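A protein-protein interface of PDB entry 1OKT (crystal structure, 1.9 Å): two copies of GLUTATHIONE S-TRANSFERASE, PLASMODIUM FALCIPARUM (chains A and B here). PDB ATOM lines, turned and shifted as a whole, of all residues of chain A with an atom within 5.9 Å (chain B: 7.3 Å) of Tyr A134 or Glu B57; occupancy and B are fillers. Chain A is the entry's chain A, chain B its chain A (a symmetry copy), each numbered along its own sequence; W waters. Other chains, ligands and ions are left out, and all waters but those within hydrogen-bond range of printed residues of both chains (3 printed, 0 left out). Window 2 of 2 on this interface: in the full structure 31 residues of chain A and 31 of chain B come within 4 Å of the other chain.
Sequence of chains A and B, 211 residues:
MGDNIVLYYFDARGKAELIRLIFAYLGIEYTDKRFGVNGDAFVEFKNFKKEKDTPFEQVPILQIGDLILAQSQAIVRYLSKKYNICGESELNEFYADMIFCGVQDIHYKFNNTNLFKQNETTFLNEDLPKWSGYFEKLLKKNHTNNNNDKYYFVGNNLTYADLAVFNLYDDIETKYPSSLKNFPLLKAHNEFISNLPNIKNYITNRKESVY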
ATOM      1  N   PRO A 129     -27.186  -5.053  10.474  1.00  0.00           N
ATOM      2  CA  PRO A 129     -26.038  -5.885  10.090  1.00  0.00           C
ATOM      3  C   PRO A 129     -24.831  -5.015   9.742  1.00  0.00           C
ATOM      4  O   PRO A 129     -23.691  -5.343  10.068  1.00  0.00           O
ATOM      5  CB  PRO A 129     -26.555  -6.652   8.870  1.00  0.00           C
ATOM      6  CG  PRO A 129     -28.016  -6.739   9.108  1.00  0.00           C
ATOM      7  CD  PRO A 129     -28.358  -5.356   9.635  1.00  0.00           C
ATOM      8  N   LYS A 130     -25.096  -3.896   9.079  1.00  0.00           N
ATOM      9  CA  LYS A 130     -24.035  -2.986   8.677  1.00  0.00           C
ATOM     10  C   LYS A 130     -23.322  -2.415   9.902  1.00  0.00           C
ATOM     11  O   LYS A 130     -22.100  -2.496  10.012  1.00  0.00           O
ATOM     12  CB  LYS A 130     -24.630  -1.873   7.814  1.00  0.00           C
ATOM     13  CG  LYS A 130     -23.617  -0.992   7.121  1.00  0.00           C
ATOM     14  CD  LYS A 130     -24.314  -0.054   6.135  1.00  0.00           C
ATOM     15  CE  LYS A 130     -25.334   0.837   6.833  1.00  0.00           C
ATOM     16  NZ  LYS A 130     -26.076   1.692   5.862  1.00  0.00           N
ATOM     17  N   TRP A 131     -24.086  -1.861  10.837  1.00  0.00           N
ATOM     18  CA  TRP A 131     -23.488  -1.295  12.043  1.00  0.00           C
ATOM     19  C   TRP A 131     -22.832  -2.338  12.948  1.00  0.00           C
ATOM     20  O   TRP A 131     -21.825  -2.057  13.591  1.00  0.00           O
ATOM     21  CB  TRP A 131     -24.525  -0.474  12.814  1.00  0.00           C
ATOM     22  CG  TRP A 131     -24.754   0.859  12.160  1.00  0.00           C
ATOM     23  CD1 TRP A 131     -25.576   1.129  11.102  1.00  0.00           C
ATOM     24  CD2 TRP A 131     -24.077   2.083  12.464  1.00  0.00           C
ATOM     25  NE1 TRP A 131     -25.448   2.447  10.722  1.00  0.00           N
ATOM     26  CE2 TRP A 131     -24.535   3.055  11.542  1.00  0.00           C
ATOM     27  CE3 TRP A 131     -23.122   2.452  13.423  1.00  0.00           C
ATOM     28  CZ2 TRP A 131     -24.075   4.379  11.555  1.00  0.00           C
ATOM     29  CZ3 TRP A 131     -22.660   3.772  13.435  1.00  0.00           C
ATOM     30  CH2 TRP A 131     -23.140   4.716  12.503  1.00  0.00           C
ATOM     31  N   SER A 132     -23.394  -3.538  13.009  1.00  0.00           N
ATOM     32  CA  SER A 132     -22.773  -4.584  13.820  1.00  0.00           C
ATOM     33  C   SER A 132     -21.379  -4.850  13.236  1.00  0.00           C
ATOM     34  O   SER A 132     -20.409  -5.049  13.971  1.00  0.00           O
ATOM     35  CB  SER A 132     -23.622  -5.859  13.801  1.00  0.00           C
ATOM     36  OG  SER A 132     -24.861  -5.649  14.454  1.00  0.00           O
ATOM     37  N   GLY A 133     -21.286  -4.827  11.907  1.00  0.00           N
ATOM     38  CA  GLY A 133     -20.012  -5.036  11.241  1.00  0.00           C
ATOM     39  C   GLY A 133     -19.032  -3.913  11.556  1.00  0.00           C
ATOM     40  O   GLY A 133     -17.832  -4.145  11.677  1.00  0.00           O
ATOM     41  N   TYR A 134     -19.529  -2.687  11.684  1.00  0.00           N
ATOM     42  CA  TYR A 134     -18.648  -1.570  12.022  1.00  0.00           C
ATOM     43  C   TYR A 134     -18.034  -1.819  13.397  1.00  0.00           C
ATOM     44  O   TYR A 134     -16.827  -1.668  13.594  1.00  0.00           O
ATOM     45  CB  TYR A 134     -19.425  -0.244  12.063  1.00  0.00           C
ATOM     46  CG  TYR A 134     -20.016   0.180  10.747  1.00  0.00           C
ATOM     47  CD1 TYR A 134     -19.387  -0.137   9.540  1.00  0.00           C
ATOM     48  CD2 TYR A 134     -21.191   0.930  10.700  1.00  0.00           C
ATOM     49  CE1 TYR A 134     -19.914   0.282   8.324  1.00  0.00           C
ATOM     50  CE2 TYR A 134     -21.725   1.353   9.490  1.00  0.00           C
ATOM     51  CZ  TYR A 134     -21.084   1.026   8.306  1.00  0.00           C
ATOM     52  OH  TYR A 134     -21.611   1.437   7.105  1.00  0.00           O
ATOM     53  N   PHE A 135     -18.876  -2.211  14.345  1.00  0.00           N
ATOM     54  CA  PHE A 135     -18.426  -2.454  15.706  1.00  0.00           C
ATOM     55  C   PHE A 135     -17.520  -3.677  15.800  1.00  0.00           C
ATOM     56  O   PHE A 135     -16.532  -3.663  16.538  1.00  0.00           O
ATOM     57  CB  PHE A 135     -19.634  -2.603  16.634  1.00  0.00           C
ATOM     58  CG  PHE A 135     -20.438  -1.332  16.787  1.00  0.00           C
ATOM     59  CD1 PHE A 135     -21.814  -1.329  16.582  1.00  0.00           C
ATOM     60  CD2 PHE A 135     -19.813  -0.141  17.154  1.00  0.00           C
ATOM     61  CE1 PHE A 135     -22.558  -0.157  16.744  1.00  0.00           C
ATOM     62  CE2 PHE A 135     -20.549   1.033  17.319  1.00  0.00           C
ATOM     63  CZ  PHE A 135     -21.921   1.022  17.114  1.00  0.00           C
ATOM     64  N   GLU A 136     -17.858  -4.730  15.056  1.00  0.00           N
ATOM     65  CA  GLU A 136     -17.050  -5.945  15.053  1.00  0.00           C
ATOM     66  C   GLU A 136     -15.622  -5.597  14.619  1.00  0.00           C
ATOM     67  O   GLU A 136     -14.654  -6.028  15.239  1.00  0.00           O
ATOM     68  CB  GLU A 136     -17.648  -6.971  14.085  1.00  0.00           C
ATOM     69  CG  GLU A 136     -16.911  -8.324  14.042  1.00  0.00           C
ATOM     70  CD  GLU A 136     -17.287  -9.239  15.195  1.00  0.00           C
ATOM     71  OE1 GLU A 136     -18.138  -8.846  16.019  1.00  0.00           O
ATOM     72  OE2 GLU A 136     -16.733 -10.358  15.281  1.00  0.00           O
ATOM     73  N   LYS A 137     -15.505  -4.810  13.552  1.00  0.00           N
ATOM     74  CA  LYS A 137     -14.210  -4.402  13.009  1.00  0.00           C
ATOM     75  C   LYS A 137     -13.429  -3.496  13.966  1.00  0.00           C
ATOM     76  O   LYS A 137     -12.202  -3.591  14.066  1.00  0.00           O
ATOM     77  CB  LYS A 137     -14.427  -3.699  11.670  1.00  0.00           C
ATOM     78  CG  LYS A 137     -13.186  -3.119  11.030  1.00  0.00           C
ATOM     79  CD  LYS A 137     -13.558  -2.479   9.705  1.00  0.00           C
ATOM     80  CE  LYS A 137     -12.399  -1.735   9.078  1.00  0.00           C
ATOM     81  NZ  LYS A 137     -12.843  -1.087   7.811  1.00  0.00           N
ATOM     82  N   LEU A 138     -14.137  -2.616  14.666  1.00  0.00           N
ATOM     83  CA  LEU A 138     -13.489  -1.719  15.619  1.00  0.00           C
ATOM     84  C   LEU A 138     -12.957  -2.520  16.801  1.00  0.00           C
ATOM     85  O   LEU A 138     -11.879  -2.250  17.317  1.00  0.00           O
ATOM     86  CB  LEU A 138     -14.481  -0.653  16.102  1.00  0.00           C
ATOM     87  CG  LEU A 138     -14.709   0.463  15.073  1.00  0.00           C
ATOM     88  CD1 LEU A 138     -15.900   1.340  15.468  1.00  0.00           C
ATOM     89  CD2 LEU A 138     -13.438   1.298  14.966  1.00  0.00           C
ATOM     90  N   LEU A 139     -13.719  -3.516  17.223  1.00  0.00           N
ATOM     91  CA  LEU A 139     -13.308  -4.355  18.338  1.00  0.00           C
ATOM     92  C   LEU A 139     -12.086  -5.170  17.901  1.00  0.00           C
ATOM     93  O   LEU A 139     -11.139  -5.365  18.669  1.00  0.00           O
ATOM     94  CB  LEU A 139     -14.478  -5.265  18.722  1.00  0.00           C
ATOM     95  CG  LEU A 139     -14.507  -6.042  20.038  1.00  0.00           C
ATOM     96  CD1 LEU A 139     -14.123  -5.156  21.215  1.00  0.00           C
ATOM     97  CD2 LEU A 139     -15.913  -6.598  20.216  1.00  0.00           C
ATOM     98  N   PHE B  45     -17.586   9.837  -3.448  1.00  0.00           N
ATOM     99  CA  PHE B  45     -17.739   9.379  -2.067  1.00  0.00           C
ATOM    100  C   PHE B  45     -17.567   7.858  -2.033  1.00  0.00           C
ATOM    101  O   PHE B  45     -16.947   7.306  -1.121  1.00  0.00           O
ATOM    102  CB  PHE B  45     -19.118   9.792  -1.529  1.00  0.00           C
ATOM    103  CG  PHE B  45     -19.391   9.339  -0.110  1.00  0.00           C
ATOM    104  CD1 PHE B  45     -18.425   9.475   0.883  1.00  0.00           C
ATOM    105  CD2 PHE B  45     -20.632   8.813   0.237  1.00  0.00           C
ATOM    106  CE1 PHE B  45     -18.686   9.098   2.194  1.00  0.00           C
ATOM    107  CE2 PHE B  45     -20.906   8.429   1.560  1.00  0.00           C
ATOM    108  CZ  PHE B  45     -19.937   8.572   2.533  1.00  0.00           C
ATOM    109  N   PHE B  48     -14.013   7.273  -2.290  1.00  0.00           N
ATOM    110  CA  PHE B  48     -13.348   7.706  -1.058  1.00  0.00           C
ATOM    111  C   PHE B  48     -13.373   6.585  -0.020  1.00  0.00           C
ATOM    112  O   PHE B  48     -12.354   6.286   0.613  1.00  0.00           O
ATOM    113  CB  PHE B  48     -14.045   8.945  -0.475  1.00  0.00           C
ATOM    114  CG  PHE B  48     -13.572   9.310   0.907  1.00  0.00           C
ATOM    115  CD1 PHE B  48     -12.356   9.966   1.097  1.00  0.00           C
ATOM    116  CD2 PHE B  48     -14.330   8.971   2.029  1.00  0.00           C
ATOM    117  CE1 PHE B  48     -11.904  10.276   2.385  1.00  0.00           C
ATOM    118  CE2 PHE B  48     -13.887   9.276   3.315  1.00  0.00           C
ATOM    119  CZ  PHE B  48     -12.672   9.929   3.494  1.00  0.00           C
ATOM    120  N   LYS B  49     -14.539   5.966   0.148  1.00  0.00           N
ATOM    121  CA  LYS B  49     -14.707   4.887   1.118  1.00  0.00           C
ATOM    122  C   LYS B  49     -13.901   3.640   0.755  1.00  0.00           C
ATOM    123  O   LYS B  49     -13.484   2.875   1.626  1.00  0.00           O
ATOM    124  CB  LYS B  49     -16.196   4.542   1.255  1.00  0.00           C
ATOM    125  CG  LYS B  49     -16.992   5.637   1.965  1.00  0.00           C
ATOM    126  CD  LYS B  49     -18.460   5.276   2.135  1.00  0.00           C
ATOM    127  CE  LYS B  49     -19.185   5.328   0.809  1.00  0.00           C
ATOM    128  NZ  LYS B  49     -20.617   4.977   0.911  1.00  0.00           N
ATOM    129  N   LYS B  50     -13.679   3.440  -0.535  1.00  0.00           N
ATOM    130  CA  LYS B  50     -12.909   2.295  -1.000  1.00  0.00           C
ATOM    131  C   LYS B  50     -11.418   2.538  -0.766  1.00  0.00           C
ATOM    132  O   LYS B  50     -10.660   1.605  -0.498  1.00  0.00           O
ATOM    133  CB  LYS B  50     -13.180   2.067  -2.489  1.00  0.00           C
ATOM    134  CG  LYS B  50     -12.310   1.011  -3.143  1.00  0.00           C
ATOM    135  CD  LYS B  50     -12.678   0.847  -4.615  1.00  0.00           C
ATOM    136  CE  LYS B  50     -11.749  -0.136  -5.319  1.00  0.00           C
ATOM    137  NZ  LYS B  50     -10.333   0.322  -5.268  1.00  0.00           N
ATOM    138  N   ASP B  53      -9.919   4.022   5.016  1.00  0.00           N
ATOM    139  CA  ASP B  53     -10.521   3.183   6.047  1.00  0.00           C
ATOM    140  C   ASP B  53     -11.348   3.974   7.064  1.00  0.00           C
ATOM    141  O   ASP B  53     -10.820   4.457   8.063  1.00  0.00           O
ATOM    142  CB  ASP B  53      -9.417   2.394   6.766  1.00  0.00           C
ATOM    143  CG  ASP B  53      -9.964   1.390   7.763  1.00  0.00           C
ATOM    144  OD1 ASP B  53     -11.017   0.786   7.476  1.00  0.00           O
ATOM    145  OD2 ASP B  53      -9.335   1.191   8.828  1.00  0.00           O
ATOM    146  N   THR B  54     -12.645   4.103   6.807  1.00  0.00           N
ATOM    147  CA  THR B  54     -13.524   4.830   7.720  1.00  0.00           C
ATOM    148  C   THR B  54     -14.207   3.828   8.648  1.00  0.00           C
ATOM    149  O   THR B  54     -14.488   2.694   8.254  1.00  0.00           O
ATOM    150  CB  THR B  54     -14.604   5.633   6.960  1.00  0.00           C
ATOM    151  OG1 THR B  54     -15.536   4.732   6.354  1.00  0.00           O
ATOM    152  CG2 THR B  54     -13.963   6.501   5.875  1.00  0.00           C
ATOM    153  N   PRO B  55     -14.476   4.229   9.902  1.00  0.00           N
ATOM    154  CA  PRO B  55     -15.126   3.335  10.861  1.00  0.00           C
ATOM    155  C   PRO B  55     -16.614   3.050  10.650  1.00  0.00           C
ATOM    156  O   PRO B  55     -17.082   1.960  10.990  1.00  0.00           O
ATOM    157  CB  PRO B  55     -14.851   4.016  12.203  1.00  0.00           C
ATOM    158  CG  PRO B  55     -14.795   5.462  11.840  1.00  0.00           C
ATOM    159  CD  PRO B  55     -13.987   5.448  10.570  1.00  0.00           C
ATOM    160  N   PHE B  56     -17.350   4.023  10.110  1.00  0.00           N
ATOM    161  CA  PHE B  56     -18.790   3.873   9.877  1.00  0.00           C
ATOM    162  C   PHE B  56     -19.250   4.297   8.486  1.00  0.00           C
ATOM    163  O   PHE B  56     -20.440   4.534   8.269  1.00  0.00           O
ATOM    164  CB  PHE B  56     -19.583   4.690  10.898  1.00  0.00           C
ATOM    165  CG  PHE B  56     -19.137   4.489  12.312  1.00  0.00           C
ATOM    166  CD1 PHE B  56     -18.497   5.511  12.996  1.00  0.00           C
ATOM    167  CD2 PHE B  56     -19.372   3.284  12.965  1.00  0.00           C
ATOM    168  CE1 PHE B  56     -18.096   5.339  14.318  1.00  0.00           C
ATOM    169  CE2 PHE B  56     -18.976   3.102  14.280  1.00  0.00           C
ATOM    170  CZ  PHE B  56     -18.337   4.136  14.961  1.00  0.00           C
ATOM    171  N   GLU B  57     -18.314   4.409   7.554  1.00  0.00           N
ATOM    172  CA  GLU B  57     -18.649   4.801   6.187  1.00  0.00           C
ATOM    173  C   GLU B  57     -19.398   6.132   6.121  1.00  0.00           C
ATOM    174  O   GLU B  57     -20.313   6.318   5.318  1.00  0.00           O
ATOM    175  CB  GLU B  57     -19.464   3.694   5.527  1.00  0.00           C
ATOM    176  CG  GLU B  57     -18.706   2.377   5.466  1.00  0.00           C
ATOM    177  CD  GLU B  57     -19.370   1.354   4.575  1.00  0.00           C
ATOM    178  OE1 GLU B  57     -20.461   0.859   4.930  1.00  0.00           O
ATOM    179  OE2 GLU B  57     -18.796   1.054   3.511  1.00  0.00           O
ATOM    180  N   GLN B  58     -18.997   7.064   6.976  1.00  0.00           N
ATOM    181  CA  GLN B  58     -19.629   8.371   6.997  1.00  0.00           C
ATOM    182  C   GLN B  58     -18.558   9.443   6.974  1.00  0.00           C
ATOM    183  O   GLN B  58     -17.392   9.186   7.278  1.00  0.00           O
ATOM    184  CB  GLN B  58     -20.448   8.577   8.279  1.00  0.00           C
ATOM    185  CG  GLN B  58     -21.530   7.543   8.584  1.00  0.00           C
ATOM    186  CD  GLN B  58     -22.197   7.824   9.919  1.00  0.00           C
ATOM    187  OE1 GLN B  58     -21.529   8.175  10.883  1.00  0.00           O
ATOM    188  NE2 GLN B  58     -23.517   7.673   9.978  1.00  0.00           N
ATOM    189  N   VAL B  59     -18.975  10.641   6.586  1.00  0.00           N
ATOM    190  CA  VAL B  59     -18.115  11.806   6.599  1.00  0.00           C
ATOM    191  C   VAL B  59     -18.938  12.779   7.449  1.00  0.00           C
ATOM    192  O   VAL B  59     -20.136  12.588   7.627  1.00  0.00           O
ATOM    193  CB  VAL B  59     -17.869  12.389   5.183  1.00  0.00           C
ATOM    194  CG1 VAL B  59     -16.863  11.520   4.443  1.00  0.00           C
ATOM    195  CG2 VAL B  59     -19.175  12.478   4.409  1.00  0.00           C
ATOM    196  N   ILE B  61     -14.687  13.296   7.689  1.00  0.00           N
ATOM    197  CA  ILE B  61     -13.530  12.521   8.094  1.00  0.00           C
ATOM    198  C   ILE B  61     -12.415  13.545   8.191  1.00  0.00           C
ATOM    199  O   ILE B  61     -12.217  14.343   7.278  1.00  0.00           O
ATOM    200  CB  ILE B  61     -13.127  11.454   7.039  1.00  0.00           C
ATOM    201  CG1 ILE B  61     -14.110  10.283   7.075  1.00  0.00           C
ATOM    202  CG2 ILE B  61     -11.706  10.953   7.317  1.00  0.00           C
ATOM    203  CD1 ILE B  61     -14.139   9.537   8.383  1.00  0.00           C
ATOM    204  N   ALA B  70     -13.268  10.179  12.771  1.00  0.00           N
ATOM    205  CA  ALA B  70     -14.642  10.232  12.265  1.00  0.00           C
ATOM    206  C   ALA B  70     -15.591  10.703  13.365  1.00  0.00           C
ATOM    207  O   ALA B  70     -15.181  10.860  14.517  1.00  0.00           O
ATOM    208  CB  ALA B  70     -15.078   8.860  11.776  1.00  0.00           C
HETATM  209  O   HOH W   1     -15.613  -0.260  11.759  1.00  0.00           O
HETATM  210  O   HOH W   2     -23.024   4.089   7.192  1.00  0.00           O
HETATM  211  O   HOH W   3     -13.527   0.850   6.363  1.00  0.00           O
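Hydrophobic or aromatic side chains of chain A that line the printed part of chain B: Trp A131, Tyr A134, Phe A135 and Leu A138.
Along chain A the printed residues that touch a printed residue of chain B span positions 131 to 138.
Of the 13 printed residues of chain B, 5 touch a printed residue of chain A.
Printed residues of chain B that touch a printed residue of chain A: Asp B53, Pro B55, Phe B56, Glu B57 and Gln B58.
Hydrophobic or aromatic side chains of chain B that line the printed part of chain A: Phe B56.
Among the printed residues, Asp or Glu carboxylates within 4 Å of a Lys or Arg side-chain nitrogen of the other chain: Lys A137 with Asp B53 (2.6 Å).
No position is printed for both chains.
Of the 8 pairs that touch across the chains among the printed residues, none has its exchanged pair printed and touching as well.
Trp A131 touches Phe B56 (CZ3 to CD2, 3.4 Å).
Trp A131 touches Gln B58.
CB of Tyr A134 touches O of Pro B55 (3.4 Å).
Tyr A134 touches Phe B56.
CE2 of Phe B56 touches CE2 of Phe A135, at 3.999 Å.
Leu A138 touches Phe B56.
OG1 of Thr B54 lies within hydrogen-bond range of N of Glu B57, at 3.0 Å.
Water W3 lies within hydrogen-bond range of the side-chain amino group of Lys A137 (2.5 Å), the side-chain carboxylate of Asp B53 (2.7 Å) and the backbone carbonyl oxygen of Thr B54 (2.8 Å).
Water W1 lies within hydrogen-bond range of O of Tyr A134 (2.6 Å) and O of Pro B55 (2.8 Å).
Water W2 lies within hydrogen-bond range of the backbone carbonyl oxygen of Phe B56 (2.8 Å) and the side-chain hydroxyl of Tyr A134 (3.0 Å).
Tyr A134 touches just these residues of chain B: Pro B55, Phe B56 and Glu B57.
Glu B57 touches just one residue of chain A: Tyr A134 (2.5 Å).
No residue of chain B comes within 4 Å of Gly A133.
Of the printed residues of chain A, Phe B56 touches Trp A131, Tyr A134, Phe A135 and Leu A138.
Of the printed residues of chain A, Pro B55 touches Tyr A134.
Phe B45 touches none of the printed residues of chain A.
Ser A132 touches none of the printed residues of chain B.
The nearest residue of chain A that does not touch Glu B57 is Lys A130 (4.1 Å).
The side-chain carboxylate (OE1) of Glu B57 is in hydrogen-bond range of the side-chain hydroxyl (OH) of Tyr A134, at 2.5 Å.
The side-chain amino group (NZ) of Lys A137 lies within salt-bridge range of the side-chain carboxylate (OD1) of Asp B53.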
